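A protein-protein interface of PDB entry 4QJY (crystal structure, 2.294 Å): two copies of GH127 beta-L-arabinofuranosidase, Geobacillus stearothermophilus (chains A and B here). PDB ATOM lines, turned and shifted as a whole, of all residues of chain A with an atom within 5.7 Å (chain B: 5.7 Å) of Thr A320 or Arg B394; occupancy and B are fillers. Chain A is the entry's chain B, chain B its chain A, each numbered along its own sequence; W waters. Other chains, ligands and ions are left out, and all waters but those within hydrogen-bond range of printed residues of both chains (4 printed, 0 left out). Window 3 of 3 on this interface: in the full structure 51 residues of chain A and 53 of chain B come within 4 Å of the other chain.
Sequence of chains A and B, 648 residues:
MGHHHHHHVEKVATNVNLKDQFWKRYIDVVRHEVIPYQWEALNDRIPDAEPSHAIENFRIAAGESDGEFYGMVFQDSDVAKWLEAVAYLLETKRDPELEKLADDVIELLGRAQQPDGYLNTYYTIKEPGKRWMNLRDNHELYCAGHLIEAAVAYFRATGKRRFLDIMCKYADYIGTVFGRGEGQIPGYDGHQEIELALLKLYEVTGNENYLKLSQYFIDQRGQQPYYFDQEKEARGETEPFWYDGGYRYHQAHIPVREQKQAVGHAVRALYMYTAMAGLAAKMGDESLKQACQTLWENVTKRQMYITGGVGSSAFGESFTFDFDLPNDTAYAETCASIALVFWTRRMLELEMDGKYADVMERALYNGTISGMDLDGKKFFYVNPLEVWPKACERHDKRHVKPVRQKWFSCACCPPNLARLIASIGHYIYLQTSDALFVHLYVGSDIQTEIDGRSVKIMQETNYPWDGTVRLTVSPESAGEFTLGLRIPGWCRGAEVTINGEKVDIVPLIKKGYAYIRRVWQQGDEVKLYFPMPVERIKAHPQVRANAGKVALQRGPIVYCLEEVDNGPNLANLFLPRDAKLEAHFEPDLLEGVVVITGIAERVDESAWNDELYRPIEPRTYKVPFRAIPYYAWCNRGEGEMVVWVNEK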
ATOM      1  N   ARG A 248     -18.333  20.649  14.080  1.00  0.00           N
ATOM      2  CA  ARG A 248     -17.087  20.036  14.471  1.00  0.00           C
ATOM      3  C   ARG A 248     -17.349  19.014  15.558  1.00  0.00           C
ATOM      4  O   ARG A 248     -16.741  17.979  15.587  1.00  0.00           O
ATOM      5  CB  ARG A 248     -16.035  21.078  14.853  1.00  0.00           C
ATOM      6  CG  ARG A 248     -15.411  21.701  13.619  1.00  0.00           C
ATOM      7  CD  ARG A 248     -14.667  23.016  13.815  1.00  0.00           C
ATOM      8  NE  ARG A 248     -13.827  22.987  15.001  1.00  0.00           N
ATOM      9  CZ  ARG A 248     -12.492  23.115  15.040  1.00  0.00           C
ATOM     10  NH1 ARG A 248     -11.764  23.335  13.940  1.00  0.00           N
ATOM     11  NH2 ARG A 248     -11.879  23.033  16.226  1.00  0.00           N
ATOM     12  N   GLN A 261      -7.416  17.219  10.970  1.00  0.00           N
ATOM     13  CA  GLN A 261      -7.218  17.472  12.381  1.00  0.00           C
ATOM     14  C   GLN A 261      -8.310  16.716  13.127  1.00  0.00           C
ATOM     15  O   GLN A 261      -9.478  16.776  12.738  1.00  0.00           O
ATOM     16  CB  GLN A 261      -7.322  18.987  12.597  1.00  0.00           C
ATOM     17  CG  GLN A 261      -7.195  19.425  14.030  1.00  0.00           C
ATOM     18  CD  GLN A 261      -5.772  19.618  14.512  1.00  0.00           C
ATOM     19  OE1 GLN A 261      -5.516  19.833  15.739  1.00  0.00           O
ATOM     20  NE2 GLN A 261      -4.830  19.548  13.581  1.00  0.00           N
ATOM     21  N   ALA A 262      -7.965  15.993  14.182  1.00  0.00           N
ATOM     22  CA  ALA A 262      -9.029  15.467  15.066  1.00  0.00           C
ATOM     23  C   ALA A 262      -9.663  16.609  15.839  1.00  0.00           C
ATOM     24  O   ALA A 262      -8.955  17.377  16.512  1.00  0.00           O
ATOM     25  CB  ALA A 262      -8.487  14.440  15.999  1.00  0.00           C
ATOM     26  N   VAL A 263     -10.993  16.731  15.704  1.00  0.00           N
ATOM     27  CA  VAL A 263     -11.817  17.730  16.371  1.00  0.00           C
ATOM     28  C   VAL A 263     -13.069  17.098  16.960  1.00  0.00           C
ATOM     29  O   VAL A 263     -13.468  16.006  16.582  1.00  0.00           O
ATOM     30  CB  VAL A 263     -12.266  18.861  15.389  1.00  0.00           C
ATOM     31  CG1 VAL A 263     -11.051  19.609  14.850  1.00  0.00           C
ATOM     32  CG2 VAL A 263     -13.127  18.351  14.251  1.00  0.00           C
ATOM     33  N   GLN A 303      -2.575  14.507  20.242  1.00  0.00           N
ATOM     34  CA  GLN A 303      -3.771  14.619  21.097  1.00  0.00           C
ATOM     35  C   GLN A 303      -4.126  13.327  21.870  1.00  0.00           C
ATOM     36  O   GLN A 303      -5.296  12.987  22.016  1.00  0.00           O
ATOM     37  CB  GLN A 303      -4.975  15.018  20.237  1.00  0.00           C
ATOM     38  CG  GLN A 303      -4.778  16.313  19.458  1.00  0.00           C
ATOM     39  CD  GLN A 303      -6.098  16.975  19.038  1.00  0.00           C
ATOM     40  OE1 GLN A 303      -6.910  17.380  19.873  1.00  0.00           O
ATOM     41  NE2 GLN A 303      -6.331  17.043  17.748  1.00  0.00           N
ATOM     42  N   SER A 312      -9.427  15.917  25.777  1.00  0.00           N
ATOM     43  CA  SER A 312      -8.790  16.771  26.764  1.00  0.00           C
ATOM     44  C   SER A 312      -9.764  17.737  27.398  1.00  0.00           C
ATOM     45  O   SER A 312      -9.378  18.450  28.327  1.00  0.00           O
ATOM     46  CB  SER A 312      -7.667  17.543  26.087  1.00  0.00           C
ATOM     47  OG  SER A 312      -8.206  18.322  24.984  1.00  0.00           O
ATOM     48  N   SER A 313     -11.019  17.778  26.944  1.00  0.00           N
ATOM     49  CA  SER A 313     -11.972  18.824  27.396  1.00  0.00           C
ATOM     50  C   SER A 313     -13.294  18.222  27.793  1.00  0.00           C
ATOM     51  O   SER A 313     -13.923  17.582  26.974  1.00  0.00           O
ATOM     52  CB  SER A 313     -12.256  19.835  26.319  1.00  0.00           C
ATOM     53  OG  SER A 313     -13.402  20.614  26.663  1.00  0.00           O
ATOM     54  N   ALA A 314     -13.703  18.452  29.042  1.00  0.00           N
ATOM     55  CA  ALA A 314     -14.967  17.958  29.556  1.00  0.00           C
ATOM     56  C   ALA A 314     -16.135  18.510  28.747  1.00  0.00           C
ATOM     57  O   ALA A 314     -17.072  17.818  28.434  1.00  0.00           O
ATOM     58  CB  ALA A 314     -15.135  18.338  31.048  1.00  0.00           C
ATOM     59  N   SER A 318     -14.376  16.362  24.347  1.00  0.00           N
ATOM     60  CA  SER A 318     -13.772  16.554  23.066  1.00  0.00           C
ATOM     61  C   SER A 318     -12.266  16.667  23.036  1.00  0.00           C
ATOM     62  O   SER A 318     -11.558  16.894  24.044  1.00  0.00           O
ATOM     63  CB  SER A 318     -14.379  17.803  22.416  1.00  0.00           C
ATOM     64  OG  SER A 318     -14.318  18.859  23.344  1.00  0.00           O
ATOM     65  N   PHE A 319     -11.781  16.510  21.810  1.00  0.00           N
ATOM     66  CA  PHE A 319     -10.449  16.966  21.413  1.00  0.00           C
ATOM     67  C   PHE A 319     -10.371  18.479  21.531  1.00  0.00           C
ATOM     68  O   PHE A 319     -11.369  19.147  21.289  1.00  0.00           O
ATOM     69  CB  PHE A 319     -10.220  16.610  19.941  1.00  0.00           C
ATOM     70  CG  PHE A 319     -10.028  15.154  19.693  1.00  0.00           C
ATOM     71  CD1 PHE A 319      -8.862  14.532  20.079  1.00  0.00           C
ATOM     72  CD2 PHE A 319     -11.014  14.408  19.082  1.00  0.00           C
ATOM     73  CE1 PHE A 319      -8.653  13.169  19.833  1.00  0.00           C
ATOM     74  CE2 PHE A 319     -10.820  13.044  18.856  1.00  0.00           C
ATOM     75  CZ  PHE A 319      -9.633  12.416  19.221  1.00  0.00           C
ATOM     76  N   THR A 320      -9.187  19.015  21.837  1.00  0.00           N
ATOM     77  CA  THR A 320      -8.952  20.462  21.750  1.00  0.00           C
ATOM     78  C   THR A 320      -8.015  20.753  20.600  1.00  0.00           C
ATOM     79  O   THR A 320      -8.458  20.932  19.491  1.00  0.00           O
ATOM     80  CB  THR A 320      -8.442  21.051  23.081  1.00  0.00           C
ATOM     81  OG1 THR A 320      -7.243  20.363  23.521  1.00  0.00           O
ATOM     82  CG2 THR A 320      -9.561  20.948  24.192  1.00  0.00           C
ATOM     83  N   PHE A 321      -6.719  20.789  20.838  1.00  0.00           N
ATOM     84  CA  PHE A 321      -5.774  21.083  19.785  1.00  0.00           C
ATOM     85  C   PHE A 321      -4.447  20.462  20.171  1.00  0.00           C
ATOM     86  O   PHE A 321      -4.240  20.003  21.298  1.00  0.00           O
ATOM     87  CB  PHE A 321      -5.634  22.601  19.568  1.00  0.00           C
ATOM     88  CG  PHE A 321      -5.267  23.339  20.825  1.00  0.00           C
ATOM     89  CD1 PHE A 321      -6.245  23.749  21.705  1.00  0.00           C
ATOM     90  CD2 PHE A 321      -3.933  23.561  21.147  1.00  0.00           C
ATOM     91  CE1 PHE A 321      -5.911  24.385  22.897  1.00  0.00           C
ATOM     92  CE2 PHE A 321      -3.585  24.179  22.348  1.00  0.00           C
ATOM     93  CZ  PHE A 321      -4.576  24.601  23.226  1.00  0.00           C
ATOM     94  N   ASP A 322      -3.567  20.421  19.194  1.00  0.00           N
ATOM     95  CA  ASP A 322      -2.270  19.755  19.307  1.00  0.00           C
ATOM     96  C   ASP A 322      -1.533  20.114  20.589  1.00  0.00           C
ATOM     97  O   ASP A 322      -1.388  21.303  20.927  1.00  0.00           O
ATOM     98  CB  ASP A 322      -1.376  20.185  18.131  1.00  0.00           C
ATOM     99  CG  ASP A 322      -1.886  19.690  16.776  1.00  0.00           C
ATOM    100  OD1 ASP A 322      -3.016  19.109  16.618  1.00  0.00           O
ATOM    101  OD2 ASP A 322      -1.120  19.926  15.850  1.00  0.00           O
ATOM    102  N   ASP A 324      -2.173  19.828  23.705  1.00  0.00           N
ATOM    103  CA  ASP A 324      -2.916  20.293  24.897  1.00  0.00           C
ATOM    104  C   ASP A 324      -3.442  19.130  25.701  1.00  0.00           C
ATOM    105  O   ASP A 324      -4.582  18.677  25.474  1.00  0.00           O
ATOM    106  CB  ASP A 324      -4.084  21.163  24.475  1.00  0.00           C
ATOM    107  CG  ASP A 324      -4.892  21.698  25.656  1.00  0.00           C
ATOM    108  OD1 ASP A 324      -4.294  22.078  26.693  1.00  0.00           O
ATOM    109  OD2 ASP A 324      -6.133  21.756  25.510  1.00  0.00           O
ATOM    110  N   PRO A 326      -3.597  18.407  29.390  1.00  0.00           N
ATOM    111  CA  PRO A 326      -3.582  18.617  30.825  1.00  0.00           C
ATOM    112  C   PRO A 326      -3.984  17.334  31.561  1.00  0.00           C
ATOM    113  O   PRO A 326      -4.884  16.581  31.136  1.00  0.00           O
ATOM    114  CB  PRO A 326      -4.644  19.683  31.032  1.00  0.00           C
ATOM    115  CG  PRO A 326      -5.597  19.451  29.911  1.00  0.00           C
ATOM    116  CD  PRO A 326      -4.772  19.026  28.759  1.00  0.00           C
ATOM    117  N   THR A 329      -7.422  18.004  34.436  1.00  0.00           N
ATOM    118  CA  THR A 329      -8.686  18.276  33.849  1.00  0.00           C
ATOM    119  C   THR A 329      -8.920  17.404  32.582  1.00  0.00           C
ATOM    120  O   THR A 329      -9.861  17.672  31.807  1.00  0.00           O
ATOM    121  CB  THR A 329      -8.715  19.726  33.391  1.00  0.00           C
ATOM    122  OG1 THR A 329      -7.602  19.955  32.511  1.00  0.00           O
ATOM    123  CG2 THR A 329      -8.652  20.671  34.574  1.00  0.00           C
ATOM    124  N   LYS B 390      -3.444  30.293  22.565  1.00  0.00           N
ATOM    125  CA  LYS B 390      -4.250  29.250  21.992  1.00  0.00           C
ATOM    126  C   LYS B 390      -5.136  28.496  23.004  1.00  0.00           C
ATOM    127  O   LYS B 390      -6.261  28.146  22.690  1.00  0.00           O
ATOM    128  CB  LYS B 390      -3.399  28.243  21.236  1.00  0.00           C
ATOM    129  CG  LYS B 390      -4.297  27.257  20.501  1.00  0.00           C
ATOM    130  CD  LYS B 390      -3.826  26.980  19.092  1.00  0.00           C
ATOM    131  CE  LYS B 390      -4.798  26.049  18.355  1.00  0.00           C
ATOM    132  NZ  LYS B 390      -6.167  26.622  18.141  1.00  0.00           N
ATOM    133  N   ALA B 391      -4.637  28.232  24.207  1.00  0.00           N
ATOM    134  CA  ALA B 391      -5.402  27.456  25.169  1.00  0.00           C
ATOM    135  C   ALA B 391      -6.520  28.249  25.816  1.00  0.00           C
ATOM    136  O   ALA B 391      -7.402  27.678  26.403  1.00  0.00           O
ATOM    137  CB  ALA B 391      -4.485  26.899  26.211  1.00  0.00           C
ATOM    138  N   CYS B 392      -6.526  29.564  25.661  1.00  0.00           N
ATOM    139  CA  CYS B 392      -7.660  30.354  26.081  1.00  0.00           C
ATOM    140  C   CYS B 392      -8.953  30.032  25.313  1.00  0.00           C
ATOM    141  O   CYS B 392     -10.012  30.536  25.672  1.00  0.00           O
ATOM    142  CB  CYS B 392      -7.300  31.860  26.010  1.00  0.00           C
ATOM    143  SG  CYS B 392      -5.868  32.280  27.100  1.00  0.00           S
ATOM    144  N   GLU B 393      -8.873  29.188  24.290  1.00  0.00           N
ATOM    145  CA  GLU B 393     -10.050  28.677  23.593  1.00  0.00           C
ATOM    146  C   GLU B 393     -10.688  27.550  24.377  1.00  0.00           C
ATOM    147  O   GLU B 393     -11.810  27.212  24.141  1.00  0.00           O
ATOM    148  CB  GLU B 393      -9.700  28.135  22.220  1.00  0.00           C
ATOM    149  CG  GLU B 393      -8.935  29.084  21.282  1.00  0.00           C
ATOM    150  CD  GLU B 393      -9.815  30.110  20.573  1.00  0.00           C
ATOM    151  OE1 GLU B 393     -11.053  30.098  20.766  1.00  0.00           O
ATOM    152  OE2 GLU B 393      -9.260  30.943  19.810  1.00  0.00           O
ATOM    153  N   ARG B 394      -9.995  26.944  25.318  1.00  0.00           N
ATOM    154  CA  ARG B 394     -10.648  25.903  26.100  1.00  0.00           C
ATOM    155  C   ARG B 394     -11.758  26.485  26.909  1.00  0.00           C
ATOM    156  O   ARG B 394     -11.634  27.593  27.420  1.00  0.00           O
ATOM    157  CB  ARG B 394      -9.688  25.253  27.055  1.00  0.00           C
ATOM    158  CG  ARG B 394      -8.593  24.450  26.397  1.00  0.00           C
ATOM    159  CD  ARG B 394      -7.645  23.990  27.503  1.00  0.00           C
ATOM    160  NE  ARG B 394      -8.396  23.226  28.507  1.00  0.00           N
ATOM    161  CZ  ARG B 394      -8.541  21.916  28.508  1.00  0.00           C
ATOM    162  NH1 ARG B 394      -7.966  21.137  27.570  1.00  0.00           N
ATOM    163  NH2 ARG B 394      -9.269  21.365  29.467  1.00  0.00           N
ATOM    164  N   HIS B 395     -12.833  25.741  27.059  1.00  0.00           N
ATOM    165  CA  HIS B 395     -13.964  26.211  27.857  1.00  0.00           C
ATOM    166  C   HIS B 395     -13.528  26.576  29.275  1.00  0.00           C
ATOM    167  O   HIS B 395     -13.967  27.579  29.831  1.00  0.00           O
ATOM    168  CB  HIS B 395     -15.021  25.108  27.891  1.00  0.00           C
ATOM    169  CG  HIS B 395     -16.322  25.493  28.518  1.00  0.00           C
ATOM    170  ND1 HIS B 395     -17.308  26.181  27.831  1.00  0.00           N
ATOM    171  CD2 HIS B 395     -16.845  25.199  29.736  1.00  0.00           C
ATOM    172  CE1 HIS B 395     -18.356  26.347  28.621  1.00  0.00           C
ATOM    173  NE2 HIS B 395     -18.099  25.771  29.785  1.00  0.00           N
ATOM    174  N   ASP B 396     -12.687  25.750  29.887  1.00  0.00           N
ATOM    175  CA  ASP B 396     -12.268  26.035  31.275  1.00  0.00           C
ATOM    176  C   ASP B 396     -11.240  27.193  31.370  1.00  0.00           C
ATOM    177  O   ASP B 396     -10.771  27.495  32.448  1.00  0.00           O
ATOM    178  CB  ASP B 396     -11.742  24.764  32.001  1.00  0.00           C
ATOM    179  CG  ASP B 396     -10.467  24.153  31.331  1.00  0.00           C
ATOM    180  OD1 ASP B 396      -9.901  24.768  30.412  1.00  0.00           O
ATOM    181  OD2 ASP B 396     -10.064  23.020  31.695  1.00  0.00           O
ATOM    182  N   LYS B 397     -10.891  27.814  30.245  1.00  0.00           N
ATOM    183  CA  LYS B 397     -10.050  29.007  30.273  1.00  0.00           C
ATOM    184  C   LYS B 397     -10.617  30.156  29.492  1.00  0.00           C
ATOM    185  O   LYS B 397      -9.906  31.110  29.196  1.00  0.00           O
ATOM    186  CB  LYS B 397      -8.686  28.717  29.716  1.00  0.00           C
ATOM    187  CG  LYS B 397      -7.876  27.819  30.600  1.00  0.00           C
ATOM    188  CD  LYS B 397      -6.532  27.499  29.950  1.00  0.00           C
ATOM    189  CE  LYS B 397      -5.962  26.271  30.649  1.00  0.00           C
ATOM    190  NZ  LYS B 397      -4.513  26.087  30.469  1.00  0.00           N
ATOM    191  N   ARG B 398     -11.892  30.100  29.157  1.00  0.00           N
ATOM    192  CA  ARG B 398     -12.420  31.124  28.260  1.00  0.00           C
ATOM    193  C   ARG B 398     -12.615  32.469  28.971  1.00  0.00           C
ATOM    194  O   ARG B 398     -12.782  33.475  28.307  1.00  0.00           O
ATOM    195  CB  ARG B 398     -13.732  30.661  27.616  1.00  0.00           C
ATOM    196  CG  ARG B 398     -14.907  30.749  28.551  1.00  0.00           C
ATOM    197  CD  ARG B 398     -16.021  29.773  28.150  1.00  0.00           C
ATOM    198  NE  ARG B 398     -17.167  29.904  29.053  1.00  0.00           N
ATOM    199  CZ  ARG B 398     -17.332  29.264  30.209  1.00  0.00           C
ATOM    200  NH1 ARG B 398     -16.445  28.378  30.660  1.00  0.00           N
ATOM    201  NH2 ARG B 398     -18.426  29.509  30.929  1.00  0.00           N
HETATM  202  O   HOH W   1      -7.152  22.585  31.762  1.00  0.00           O
HETATM  203  O   HOH W   2     -11.697  19.564  30.742  1.00  0.00           O
HETATM  204  O   HOH W   3      -5.436  22.970  29.479  1.00  0.00           O
HETATM  205  O   HOH W   4     -13.041  23.143  25.497  1.00  0.00           O
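The guanidinium group of Arg B394 lies within salt-bridge range of the side-chain carboxylate of Asp B396 (2.9 Å). N of Ser A312 sits at hydrogen-bond distance from O of Ser A318. The side-chain hydroxyl (OG1) of Thr A320 sits at hydrogen-bond distance from the side-chain carboxylate (OD2) of Asp A324 (2.7 Å). The side-chain amide oxygen (OE1) of Gln A303 lies within hydrogen-bond range of the backbone NH (N) of Thr A320, 3.4 Å away. The side-chain hydroxyl (OG) of Ser A312 is in hydrogen-bond range of the side-chain hydroxyl (OG1) of Thr A320.
Water W1 lies within hydrogen-bond range of OG1 of Thr A329 (2.8 Å), OD2 of Asp B396 (2.9 Å) and NH2 of Arg B394 (3.4 Å). Water W4 lies within hydrogen-bond range of OG of Ser A313 (2.8 Å) and N of His B395 (3.0 Å). Water W2 lies within hydrogen-bond range of O of Thr A329, N of Ala A314 and NH2 of Arg B394. Water W3 lies within hydrogen-bond range of the guanidinium group of Arg B394 (3.1 Å), the side-chain carboxylate of Asp A324 (3.1 Å) and the side-chain amino group of Lys B397 (3.4 Å).
Printed residues of chain B within 4 Å of Ser A312: Arg B394 (3.1 Å). Thr A320 touches one residue of chain B. Of chain A, only Ser A312, Thr A320, Asp A324, Pro A326 and Thr A329 come within 4 Å of Arg B394. Of the printed residues of chain A, Asp B396 touches Thr A329 (3.9 Å). The nearest residue of chain A that does not touch Arg B394 is Ser A313 (4.2 Å). The nearest printed residue of chain A that does not touch Lys B390 is Asp A322 (5.8 Å).
The guanidinium group (NH1) of Arg B394 is in hydrogen-bond range of the backbone carbonyl oxygen (O) of Ser A312, at 3.1 Å. The side-chain carboxylate (OD2) of Asp A324 lies within salt-bridge range of the guanidinium group (NH1) of Arg B394 (2.8 Å).
No position is printed for both chains. Of the 8 pairs that touch across the chains among the printed residues, none has its exchanged pair printed and touching as well.
CG2 of Thr A320 touches NH1 of Arg B394 (3.7 Å). CE2 of Phe A321 touches CG of Lys B390, at 3.7 Å. CZ of Phe A321 touches CA of Ala B391, at 3.6 Å. Arg B394 touches Pro A326 (NH1 to CG, 3.7 Å). Thr A329 touches Arg B394. Asp B396 touches Thr A329 (OD2 to CB, 3.9 Å).
Hydrophobic or aromatic side chains of chain A within 4 Å of the printed part of chain B: Phe A321 and Pro A326.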
